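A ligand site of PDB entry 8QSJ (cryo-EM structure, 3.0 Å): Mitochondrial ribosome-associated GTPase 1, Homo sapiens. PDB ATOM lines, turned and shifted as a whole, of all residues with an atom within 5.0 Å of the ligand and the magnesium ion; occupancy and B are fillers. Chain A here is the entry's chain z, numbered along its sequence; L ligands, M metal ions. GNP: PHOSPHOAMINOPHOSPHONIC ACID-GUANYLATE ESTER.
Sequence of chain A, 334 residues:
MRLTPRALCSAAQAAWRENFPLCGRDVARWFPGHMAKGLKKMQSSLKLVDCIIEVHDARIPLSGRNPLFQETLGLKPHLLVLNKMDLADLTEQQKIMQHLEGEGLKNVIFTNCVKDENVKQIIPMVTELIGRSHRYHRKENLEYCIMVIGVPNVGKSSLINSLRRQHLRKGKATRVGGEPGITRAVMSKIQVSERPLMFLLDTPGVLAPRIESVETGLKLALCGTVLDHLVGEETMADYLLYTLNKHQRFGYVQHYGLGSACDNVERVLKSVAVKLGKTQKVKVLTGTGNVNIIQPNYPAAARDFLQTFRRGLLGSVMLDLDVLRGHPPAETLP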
ATOM      1  N   ASN A  83     -16.074 -23.788  -5.810  1.00  0.00           N
ATOM      2  CA  ASN A  83     -14.842 -23.361  -6.436  1.00  0.00           C
ATOM      3  C   ASN A  83     -15.132 -22.509  -7.677  1.00  0.00           C
ATOM      4  O   ASN A  83     -16.267 -22.417  -8.146  1.00  0.00           O
ATOM      5  CB  ASN A  83     -13.987 -24.572  -6.814  1.00  0.00           C
ATOM      6  CG  ASN A  83     -12.530 -24.212  -7.026  1.00  0.00           C
ATOM      7  OD1 ASN A  83     -12.082 -23.142  -6.640  1.00  0.00           O
ATOM      8  ND2 ASN A  83     -11.781 -25.127  -7.632  1.00  0.00           N
ATOM      9  N   LYS A  84     -14.081 -21.887  -8.200  1.00  0.00           N
ATOM     10  CA  LYS A  84     -14.135 -21.072  -9.412  1.00  0.00           C
ATOM     11  C   LYS A  84     -15.118 -19.910  -9.255  1.00  0.00           C
ATOM     12  O   LYS A  84     -16.080 -19.760 -10.010  1.00  0.00           O
ATOM     13  CB  LYS A  84     -14.479 -21.929 -10.635  1.00  0.00           C
ATOM     14  CG  LYS A  84     -13.847 -23.309 -10.659  1.00  0.00           C
ATOM     15  CD  LYS A  84     -12.782 -23.417 -11.735  1.00  0.00           C
ATOM     16  CE  LYS A  84     -12.295 -24.855 -11.890  1.00  0.00           C
ATOM     17  NZ  LYS A  84     -12.213 -25.265 -13.316  1.00  0.00           N
ATOM     18  N   MET A  85     -14.850 -19.077  -8.243  1.00  0.00           N
ATOM     19  CA  MET A  85     -15.675 -17.898  -8.032  1.00  0.00           C
ATOM     20  C   MET A  85     -15.435 -16.847  -9.106  1.00  0.00           C
ATOM     21  O   MET A  85     -16.358 -16.097  -9.454  1.00  0.00           O
ATOM     22  CB  MET A  85     -15.416 -17.296  -6.654  1.00  0.00           C
ATOM     23  CG  MET A  85     -13.963 -16.926  -6.416  1.00  0.00           C
ATOM     24  SD  MET A  85     -13.641 -16.339  -4.738  1.00  0.00           S
ATOM     25  CE  MET A  85     -14.916 -17.202  -3.832  1.00  0.00           C
ATOM     26  N   ASP A  86     -14.214 -16.775  -9.640  1.00  0.00           N
ATOM     27  CA  ASP A  86     -13.893 -15.780 -10.646  1.00  0.00           C
ATOM     28  C   ASP A  86     -14.740 -15.958 -11.907  1.00  0.00           C
ATOM     29  O   ASP A  86     -15.101 -14.973 -12.550  1.00  0.00           O
ATOM     30  CB  ASP A  86     -12.409 -15.851 -11.002  1.00  0.00           C
ATOM     31  CG  ASP A  86     -11.964 -17.245 -11.375  1.00  0.00           C
ATOM     32  OD1 ASP A  86     -12.633 -18.222 -10.959  1.00  0.00           O
ATOM     33  OD2 ASP A  86     -10.945 -17.378 -12.087  1.00  0.00           O
ATOM     34  N   LEU A  87     -15.054 -17.199 -12.258  1.00  0.00           N
ATOM     35  CA  LEU A  87     -15.844 -17.487 -13.442  1.00  0.00           C
ATOM     36  C   LEU A  87     -17.342 -17.451 -13.179  1.00  0.00           C
ATOM     37  O   LEU A  87     -18.137 -17.667 -14.105  1.00  0.00           O
ATOM     38  CB  LEU A  87     -15.459 -18.862 -14.005  1.00  0.00           C
ATOM     39  CG  LEU A  87     -13.959 -19.136 -14.149  1.00  0.00           C
ATOM     40  CD1 LEU A  87     -13.728 -20.493 -14.811  1.00  0.00           C
ATOM     41  CD2 LEU A  87     -13.274 -18.034 -14.938  1.00  0.00           C
ATOM     42  N   THR A 111     -14.874 -20.477  -2.790  1.00  0.00           N
ATOM     43  CA  THR A 111     -13.421 -20.470  -2.786  1.00  0.00           C
ATOM     44  C   THR A 111     -12.891 -20.214  -4.186  1.00  0.00           C
ATOM     45  O   THR A 111     -13.608 -20.332  -5.181  1.00  0.00           O
ATOM     46  CB  THR A 111     -12.845 -21.789  -2.252  1.00  0.00           C
ATOM     47  OG1 THR A 111     -11.463 -21.615  -1.937  1.00  0.00           O
ATOM     48  CG2 THR A 111     -12.986 -22.889  -3.283  1.00  0.00           C
ATOM     49  N   ASN A 112     -11.608 -19.845  -4.239  1.00  0.00           N
ATOM     50  CA  ASN A 112     -10.884 -19.596  -5.494  1.00  0.00           C
ATOM     51  C   ASN A 112      -9.589 -20.398  -5.425  1.00  0.00           C
ATOM     52  O   ASN A 112      -8.623 -19.974  -4.776  1.00  0.00           O
ATOM     53  CB  ASN A 112     -10.627 -18.102  -5.675  1.00  0.00           C
ATOM     54  CG  ASN A 112      -9.926 -17.783  -6.977  1.00  0.00           C
ATOM     55  OD1 ASN A 112      -9.607 -18.661  -7.773  1.00  0.00           O
ATOM     56  ND2 ASN A 112      -9.695 -16.487  -7.223  1.00  0.00           N
ATOM     57  N   CYS A 113      -9.562 -21.551  -6.088  1.00  0.00           N
ATOM     58  CA  CYS A 113      -8.428 -22.455  -5.958  1.00  0.00           C
ATOM     59  C   CYS A 113      -7.195 -21.936  -6.683  1.00  0.00           C
ATOM     60  O   CYS A 113      -6.071 -22.122  -6.202  1.00  0.00           O
ATOM     61  CB  CYS A 113      -8.795 -23.848  -6.462  1.00  0.00           C
ATOM     62  SG  CYS A 113      -9.695 -24.856  -5.275  1.00  0.00           S
ATOM     63  N   VAL A 114      -7.373 -21.306  -7.851  1.00  0.00           N
ATOM     64  CA  VAL A 114      -6.222 -20.820  -8.596  1.00  0.00           C
ATOM     65  C   VAL A 114      -5.536 -19.656  -7.891  1.00  0.00           C
ATOM     66  O   VAL A 114      -4.367 -19.361  -8.180  1.00  0.00           O
ATOM     67  CB  VAL A 114      -6.646 -20.430 -10.029  1.00  0.00           C
ATOM     68  CG1 VAL A 114      -7.346 -19.077 -10.027  1.00  0.00           C
ATOM     69  CG2 VAL A 114      -5.441 -20.419 -10.961  1.00  0.00           C
ATOM     70  N   VAL A 151     -17.757 -33.668  -8.865  1.00  0.00           N
ATOM     71  CA  VAL A 151     -17.763 -34.095 -10.256  1.00  0.00           C
ATOM     72  C   VAL A 151     -16.394 -33.762 -10.846  1.00  0.00           C
ATOM     73  O   VAL A 151     -15.648 -32.961 -10.255  1.00  0.00           O
ATOM     74  CB  VAL A 151     -18.910 -33.453 -11.052  1.00  0.00           C
ATOM     75  CG1 VAL A 151     -20.257 -33.982 -10.557  1.00  0.00           C
ATOM     76  CG2 VAL A 151     -18.864 -31.939 -10.962  1.00  0.00           C
ATOM     77  N   PRO A 152     -15.998 -34.353 -11.972  1.00  0.00           N
ATOM     78  CA  PRO A 152     -14.665 -34.074 -12.523  1.00  0.00           C
ATOM     79  C   PRO A 152     -14.488 -32.598 -12.861  1.00  0.00           C
ATOM     80  O   PRO A 152     -15.432 -31.895 -13.222  1.00  0.00           O
ATOM     81  CB  PRO A 152     -14.604 -34.951 -13.775  1.00  0.00           C
ATOM     82  CG  PRO A 152     -15.571 -36.036 -13.530  1.00  0.00           C
ATOM     83  CD  PRO A 152     -16.683 -35.414 -12.731  1.00  0.00           C
ATOM     84  N   ASN A 153     -13.238 -32.140 -12.721  1.00  0.00           N
ATOM     85  CA  ASN A 153     -12.825 -30.781 -13.099  1.00  0.00           C
ATOM     86  C   ASN A 153     -13.618 -29.717 -12.330  1.00  0.00           C
ATOM     87  O   ASN A 153     -14.377 -28.942 -12.895  1.00  0.00           O
ATOM     88  CB  ASN A 153     -12.949 -30.574 -14.611  1.00  0.00           C
ATOM     89  CG  ASN A 153     -11.979 -29.544 -15.132  1.00  0.00           C
ATOM     90  OD1 ASN A 153     -12.050 -28.368 -14.779  1.00  0.00           O
ATOM     91  ND2 ASN A 153     -11.048 -29.976 -15.976  1.00  0.00           N
ATOM     92  N   VAL A 154     -13.411 -29.715 -11.011  1.00  0.00           N
ATOM     93  CA  VAL A 154     -13.972 -28.660 -10.164  1.00  0.00           C
ATOM     94  C   VAL A 154     -12.870 -28.099  -9.285  1.00  0.00           C
ATOM     95  O   VAL A 154     -13.054 -27.090  -8.606  1.00  0.00           O
ATOM     96  CB  VAL A 154     -15.139 -29.192  -9.307  1.00  0.00           C
ATOM     97  CG1 VAL A 154     -16.358 -29.448 -10.168  1.00  0.00           C
ATOM     98  CG2 VAL A 154     -14.721 -30.446  -8.560  1.00  0.00           C
ATOM     99  N   GLY A 155     -11.703 -28.746  -9.307  1.00  0.00           N
ATOM    100  CA  GLY A 155     -10.574 -28.307  -8.510  1.00  0.00           C
ATOM    101  C   GLY A 155     -10.289 -29.146  -7.280  1.00  0.00           C
ATOM    102  O   GLY A 155      -9.701 -28.611  -6.338  1.00  0.00           O
ATOM    103  N   LYS A 156     -10.687 -30.414  -7.269  1.00  0.00           N
ATOM    104  CA  LYS A 156     -10.422 -31.257  -6.095  1.00  0.00           C
ATOM    105  C   LYS A 156      -8.924 -31.404  -5.860  1.00  0.00           C
ATOM    106  O   LYS A 156      -8.444 -31.238  -4.729  1.00  0.00           O
ATOM    107  CB  LYS A 156     -11.078 -32.632  -6.291  1.00  0.00           C
ATOM    108  CG  LYS A 156     -12.584 -32.584  -6.449  1.00  0.00           C
ATOM    109  CD  LYS A 156     -13.152 -33.959  -6.742  1.00  0.00           C
ATOM    110  CE  LYS A 156     -12.570 -34.531  -8.032  1.00  0.00           C
ATOM    111  NZ  LYS A 156     -12.868 -33.657  -9.201  1.00  0.00           N
ATOM    112  N   SER A 157      -8.167 -31.719  -6.912  1.00  0.00           N
ATOM    113  CA  SER A 157      -6.716 -31.790  -6.777  1.00  0.00           C
ATOM    114  C   SER A 157      -6.134 -30.410  -6.486  1.00  0.00           C
ATOM    115  O   SER A 157      -5.184 -30.290  -5.696  1.00  0.00           O
ATOM    116  CB  SER A 157      -6.102 -32.380  -8.040  1.00  0.00           C
ATOM    117  OG  SER A 157      -6.710 -33.616  -8.371  1.00  0.00           O
ATOM    118  N   SER A 158      -6.674 -29.362  -7.103  1.00  0.00           N
ATOM    119  CA  SER A 158      -6.201 -28.009  -6.848  1.00  0.00           C
ATOM    120  C   SER A 158      -6.475 -27.604  -5.401  1.00  0.00           C
ATOM    121  O   SER A 158      -5.662 -26.897  -4.782  1.00  0.00           O
ATOM    122  CB  SER A 158      -6.848 -27.025  -7.811  1.00  0.00           C
ATOM    123  OG  SER A 158      -6.346 -25.710  -7.620  1.00  0.00           O
ATOM    124  N   ARG A 175      -1.449 -34.143  -9.283  1.00  0.00           N
ATOM    125  CA  ARG A 175      -1.460 -33.662 -10.659  1.00  0.00           C
ATOM    126  C   ARG A 175      -2.725 -32.862 -10.932  1.00  0.00           C
ATOM    127  O   ARG A 175      -3.831 -33.285 -10.571  1.00  0.00           O
ATOM    128  CB  ARG A 175      -1.340 -34.819 -11.641  1.00  0.00           C
ATOM    129  CG  ARG A 175      -1.306 -34.387 -13.102  1.00  0.00           C
ATOM    130  CD  ARG A 175      -1.007 -35.556 -14.018  1.00  0.00           C
ATOM    131  NE  ARG A 175       0.351 -36.053 -13.871  1.00  0.00           N
ATOM    132  CZ  ARG A 175       0.890 -36.999 -14.626  1.00  0.00           C
ATOM    133  NH1 ARG A 175       0.197 -37.585 -15.588  1.00  0.00           N
ATOM    134  NH2 ARG A 175       2.148 -37.364 -14.404  1.00  0.00           N
ATOM    135  N   VAL A 176      -2.563 -31.712 -11.575  1.00  0.00           N
ATOM    136  CA  VAL A 176      -3.662 -30.814 -11.881  1.00  0.00           C
ATOM    137  C   VAL A 176      -3.663 -30.546 -13.383  1.00  0.00           C
ATOM    138  O   VAL A 176      -2.618 -30.209 -13.948  1.00  0.00           O
ATOM    139  CB  VAL A 176      -3.564 -29.488 -11.098  1.00  0.00           C
ATOM    140  CG1 VAL A 176      -4.498 -28.451 -11.679  1.00  0.00           C
ATOM    141  CG2 VAL A 176      -3.883 -29.723  -9.631  1.00  0.00           C
ATOM    142  N   GLY A 177      -4.828 -30.715 -14.017  1.00  0.00           N
ATOM    143  CA  GLY A 177      -4.946 -30.474 -15.443  1.00  0.00           C
ATOM    144  C   GLY A 177      -6.258 -29.814 -15.779  1.00  0.00           C
ATOM    145  O   GLY A 177      -7.172 -29.727 -14.963  1.00  0.00           O
ATOM    146  N   GLY A 178      -6.343 -29.338 -17.024  1.00  0.00           N
ATOM    147  CA  GLY A 178      -7.540 -28.686 -17.508  1.00  0.00           C
ATOM    148  C   GLY A 178      -8.449 -29.614 -18.277  1.00  0.00           C
ATOM    149  O   GLY A 178      -9.311 -29.158 -19.034  1.00  0.00           O
ATOM    150  N   GLU A 179      -8.267 -30.919 -18.091  1.00  0.00           N
ATOM    151  CA  GLU A 179      -9.057 -31.923 -18.788  1.00  0.00           C
ATOM    152  C   GLU A 179      -9.791 -32.804 -17.790  1.00  0.00           C
ATOM    153  O   GLU A 179      -9.294 -33.041 -16.678  1.00  0.00           O
ATOM    154  CB  GLU A 179      -8.150 -32.798 -19.673  1.00  0.00           C
ATOM    155  CG  GLU A 179      -8.772 -33.162 -21.014  1.00  0.00           C
ATOM    156  CD  GLU A 179      -7.720 -33.548 -22.041  1.00  0.00           C
ATOM    157  OE1 GLU A 179      -7.250 -32.644 -22.763  1.00  0.00           O
ATOM    158  OE2 GLU A 179      -7.376 -34.745 -22.135  1.00  0.00           O
ATOM    159  N   PRO A 180     -10.978 -33.294 -18.140  1.00  0.00           N
ATOM    160  CA  PRO A 180     -11.686 -34.224 -17.253  1.00  0.00           C
ATOM    161  C   PRO A 180     -10.915 -35.531 -17.090  1.00  0.00           C
ATOM    162  O   PRO A 180     -10.225 -35.990 -18.012  1.00  0.00           O
ATOM    163  CB  PRO A 180     -13.025 -34.453 -17.960  1.00  0.00           C
ATOM    164  CG  PRO A 180     -13.193 -33.270 -18.857  1.00  0.00           C
ATOM    165  CD  PRO A 180     -11.817 -32.881 -19.283  1.00  0.00           C
ATOM    166  N   GLY A 181     -11.038 -36.123 -15.917  1.00  0.00           N
ATOM    167  CA  GLY A 181     -10.404 -37.395 -15.648  1.00  0.00           C
ATOM    168  C   GLY A 181      -8.911 -37.355 -15.389  1.00  0.00           C
ATOM    169  O   GLY A 181      -8.209 -38.317 -15.709  1.00  0.00           O
ATOM    170  N   ILE A 182      -8.410 -36.248 -14.829  1.00  0.00           N
ATOM    171  CA  ILE A 182      -6.981 -36.164 -14.527  1.00  0.00           C
ATOM    172  C   ILE A 182      -6.614 -37.141 -13.414  1.00  0.00           C
ATOM    173  O   ILE A 182      -5.650 -37.906 -13.532  1.00  0.00           O
ATOM    174  CB  ILE A 182      -6.596 -34.719 -14.155  1.00  0.00           C
ATOM    175  CG1 ILE A 182      -6.482 -33.865 -15.428  1.00  0.00           C
ATOM    176  CG2 ILE A 182      -5.299 -34.699 -13.371  1.00  0.00           C
ATOM    177  CD1 ILE A 182      -5.185 -34.068 -16.179  1.00  0.00           C
ATOM    178  N   THR A 183      -7.385 -37.152 -12.337  1.00  0.00           N
ATOM    179  CA  THR A 183      -7.173 -38.082 -11.229  1.00  0.00           C
ATOM    180  C   THR A 183      -7.894 -39.380 -11.551  1.00  0.00           C
ATOM    181  O   THR A 183      -9.125 -39.461 -11.450  1.00  0.00           O
ATOM    182  CB  THR A 183      -7.652 -37.471  -9.914  1.00  0.00           C
ATOM    183  OG1 THR A 183      -7.073 -36.182  -9.736  1.00  0.00           O
ATOM    184  CG2 THR A 183      -7.262 -38.368  -8.746  1.00  0.00           C
ATOM    185  N   ASP A 202      -7.311 -37.592  -2.262  1.00  0.00           N
ATOM    186  CA  ASP A 202      -7.661 -37.195  -3.627  1.00  0.00           C
ATOM    187  C   ASP A 202      -8.455 -38.305  -4.301  1.00  0.00           C
ATOM    188  O   ASP A 202      -8.024 -39.469  -4.331  1.00  0.00           O
ATOM    189  CB  ASP A 202      -6.403 -36.875  -4.434  1.00  0.00           C
ATOM    190  CG  ASP A 202      -6.698 -35.947  -5.599  1.00  0.00           C
ATOM    191  OD1 ASP A 202      -7.879 -35.597  -5.788  1.00  0.00           O
ATOM    192  OD2 ASP A 202      -5.746 -35.568  -6.314  1.00  0.00           O
ATOM    193  N   THR A 203      -9.609 -37.952  -4.839  1.00  0.00           N
ATOM    194  CA  THR A 203     -10.525 -38.923  -5.410  1.00  0.00           C
ATOM    195  C   THR A 203     -10.946 -38.488  -6.805  1.00  0.00           C
ATOM    196  O   THR A 203     -11.002 -37.289  -7.089  1.00  0.00           O
ATOM    197  CB  THR A 203     -11.778 -39.067  -4.525  1.00  0.00           C
ATOM    198  OG1 THR A 203     -12.551 -37.865  -4.583  1.00  0.00           O
ATOM    199  CG2 THR A 203     -11.367 -39.312  -3.082  1.00  0.00           C
ATOM    200  N   PRO A 204     -11.232 -39.437  -7.690  1.00  0.00           N
ATOM    201  CA  PRO A 204     -11.683 -39.068  -9.034  1.00  0.00           C
ATOM    202  C   PRO A 204     -13.036 -38.388  -9.006  1.00  0.00           C
ATOM    203  O   PRO A 204     -13.874 -38.651  -8.128  1.00  0.00           O
ATOM    204  CB  PRO A 204     -11.757 -40.407  -9.781  1.00  0.00           C
ATOM    205  CG  PRO A 204     -10.999 -41.378  -8.932  1.00  0.00           C
ATOM    206  CD  PRO A 204     -11.127 -40.891  -7.526  1.00  0.00           C
ATOM    207  N   GLY A 205     -13.249 -37.489  -9.958  1.00  0.00           N
ATOM    208  CA  GLY A 205     -14.564 -36.888 -10.115  1.00  0.00           C
ATOM    209  C   GLY A 205     -15.574 -37.934 -10.565  1.00  0.00           C
ATOM    210  O   GLY A 205     -15.296 -38.748 -11.450  1.00  0.00           O
HETATM  211  PG  GNP L   1     -10.261 -34.427 -12.062  1.00  0.00           P
HETATM  212  O1G GNP L   1     -10.545 -34.940 -13.439  1.00  0.00           O
HETATM  213  O2G GNP L   1      -8.881 -34.909 -11.615  1.00  0.00           O
HETATM  214  O3G GNP L   1     -11.341 -34.972 -11.085  1.00  0.00           O
HETATM  215  N3B GNP L   1     -10.310 -32.725 -12.062  1.00  0.00           N
HETATM  216  PB  GNP L   1      -9.859 -31.895 -10.726  1.00  0.00           P
HETATM  217  O1B GNP L   1     -10.886 -32.072  -9.634  1.00  0.00           O
HETATM  218  O2B GNP L   1      -8.526 -32.401 -10.246  1.00  0.00           O
HETATM  219  O3A GNP L   1      -9.703 -30.303 -11.074  1.00  0.00           O
HETATM  220  PA  GNP L   1      -8.292 -29.591 -11.156  1.00  0.00           P
HETATM  221  O1A GNP L   1      -7.774 -29.449  -9.722  1.00  0.00           O
HETATM  222  O2A GNP L   1      -7.377 -30.312 -12.077  1.00  0.00           O
HETATM  223  O5' GNP L   1      -8.631 -28.169 -11.737  1.00  0.00           O
HETATM  224  C5' GNP L   1      -9.232 -28.017 -13.030  1.00  0.00           C
HETATM  225  C4' GNP L   1      -8.593 -26.849 -13.753  1.00  0.00           C
HETATM  226  O4' GNP L   1      -9.237 -25.620 -13.339  1.00  0.00           O
HETATM  227  C3' GNP L   1      -7.100 -26.665 -13.502  1.00  0.00           C
HETATM  228  O3' GNP L   1      -6.431 -26.266 -14.694  1.00  0.00           O
HETATM  229  C2' GNP L   1      -7.061 -25.564 -12.436  1.00  0.00           C
HETATM  230  O2' GNP L   1      -5.877 -24.788 -12.513  1.00  0.00           O
HETATM  231  C1' GNP L   1      -8.272 -24.723 -12.836  1.00  0.00           C
HETATM  232  N9  GNP L   1      -8.874 -23.998 -11.695  1.00  0.00           N
HETATM  233  C8  GNP L   1      -9.106 -24.495 -10.444  1.00  0.00           C
HETATM  234  N7  GNP L   1      -9.659 -23.621  -9.642  1.00  0.00           N
HETATM  235  C5  GNP L   1      -9.789 -22.480 -10.415  1.00  0.00           C
HETATM  236  C6  GNP L   1     -10.341 -21.183 -10.100  1.00  0.00           C
HETATM  237  O6  GNP L   1     -10.807 -20.809  -9.025  1.00  0.00           O
HETATM  238  N1  GNP L   1     -10.284 -20.321 -11.185  1.00  0.00           N
HETATM  239  C2  GNP L   1      -9.788 -20.642 -12.422  1.00  0.00           C
HETATM  240  N2  GNP L   1      -9.814 -19.688 -13.348  1.00  0.00           N
HETATM  241  N3  GNP L   1      -9.285 -21.840 -12.723  1.00  0.00           N
HETATM  242  C4  GNP L   1      -9.318 -22.703 -11.687  1.00  0.00           C
HETATM  243 MG    MG M   1      -7.787 -34.276  -9.994  1.00  0.00          MG
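The magnesium ion is bound by O2B of the ligand, OG1 of Thr 183, O2G of the ligand and OG of Ser 157. The magnesium ion has four donor atoms within binding distance.
O1B of the ligand is in hydrogen-bond range of N of Lys 156 (2.9 Å). N of Gly 177 lies within hydrogen-bond range of O2A of the ligand (3.2 Å). N of Ser 157 lies close to O2B of the ligand, at 3.4 Å. An oxygen (O4') of the ligand is in hydrogen-bond range of the side-chain amino group (NZ) of Lys 84. An oxygen (O1A) of the ligand sits at hydrogen-bond distance from the backbone NH of Ser 158, at 2.8 Å. N of Cys 113 is in hydrogen-bond range of O6 of the ligand (3.3 Å). N of Gly 181 lies within hydrogen-bond range of O1G of the ligand (2.8 Å). N of Gly 155 sits at hydrogen-bond distance from O3A of the ligand, at 3.1 Å. An oxygen (O1B) of the ligand lies within salt-bridge range of the side-chain amino group (NZ) of Lys 156, 2.6 Å away. An oxygen (O3G) of the ligand sits at hydrogen-bond distance from the backbone NH (N) of Gly 205, 3.4 Å away. The backbone NH (N) of Thr 183 sits close to an oxygen (O2G) of the ligand. OD1 of Asn 112 lies close to O6 of the ligand (2.8 Å). ND2 of Asn 83 sits at hydrogen-bond distance from N7 of the ligand (3.3 Å). The backbone carbonyl oxygen (O) of Gly 177 lies close to an oxygen (O2A) of the ligand, 3.0 Å away. The side-chain carboxylate (OD2) of Asp 86 sits at hydrogen-bond distance from a nitrogen (N2) of the ligand, 2.9 Å away. N of Ile 182 sits at hydrogen-bond distance from O1G of the ligand (2.9 Å).
The backbone NH (N) of Asn 153 sits close to a nitrogen (N3B) of the ligand (3.1 Å). Residues that only touch the ligand: Val 114 (3.4 Å), Val 176 (3.5 Å), Pro 180 (3.7 Å), Val 154 (3.7 Å), Pro 152 (3.7 Å), Gly 178 (3.9 Å) and Glu 179 (3.96 Å). Hydrophobic or aromatic side chains that line the ligand: Val 114, Val 176 and Ile 182. Within 4 Å of the ligand: Asn 83, Lys 84, Asp 86, Asn 112, Cys 113, Val 114, Pro 152, Asn 153, Val 154, Gly 155, Lys 156, Ser 157, Ser 158, Val 176, Gly 177, Gly 178, Glu 179, Pro 180, Gly 181, Ile 182, Thr 183 and Gly 205. The nearest printed residue that does not touch the ligand is Leu 87 (4.2 Å).
The side-chain amino group (NZ) of Lys 84 is in hydrogen-bond range of the side-chain amide oxygen (OD1) of Asn 153, at 3.4 Å. The side-chain amide oxygen (OD1) of Asn 112 sits close to the backbone NH (N) of Val 114, 3.5 Å away. The side-chain amide nitrogen (ND2) of Asn 83 is in hydrogen-bond range of the backbone carbonyl oxygen (O) of Val 154, 2.5 Å away. N of Lys 84 lies within hydrogen-bond range of O of Thr 111 (3.4 Å). The side-chain hydroxyl (OG) of Ser 157 sits close to the side-chain carboxylate (OD2) of Asp 202 (3.0 Å). The side-chain amide oxygen of Asn 83 lies within hydrogen-bond range of the backbone NH of Cys 113 (3.0 Å). The side-chain amino group of Lys 156 is in hydrogen-bond range of the backbone carbonyl oxygen of Val 151 (3.1 Å).
The nearest printed residue that does not touch the magnesium ion is Arg 175 (4.1 Å).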
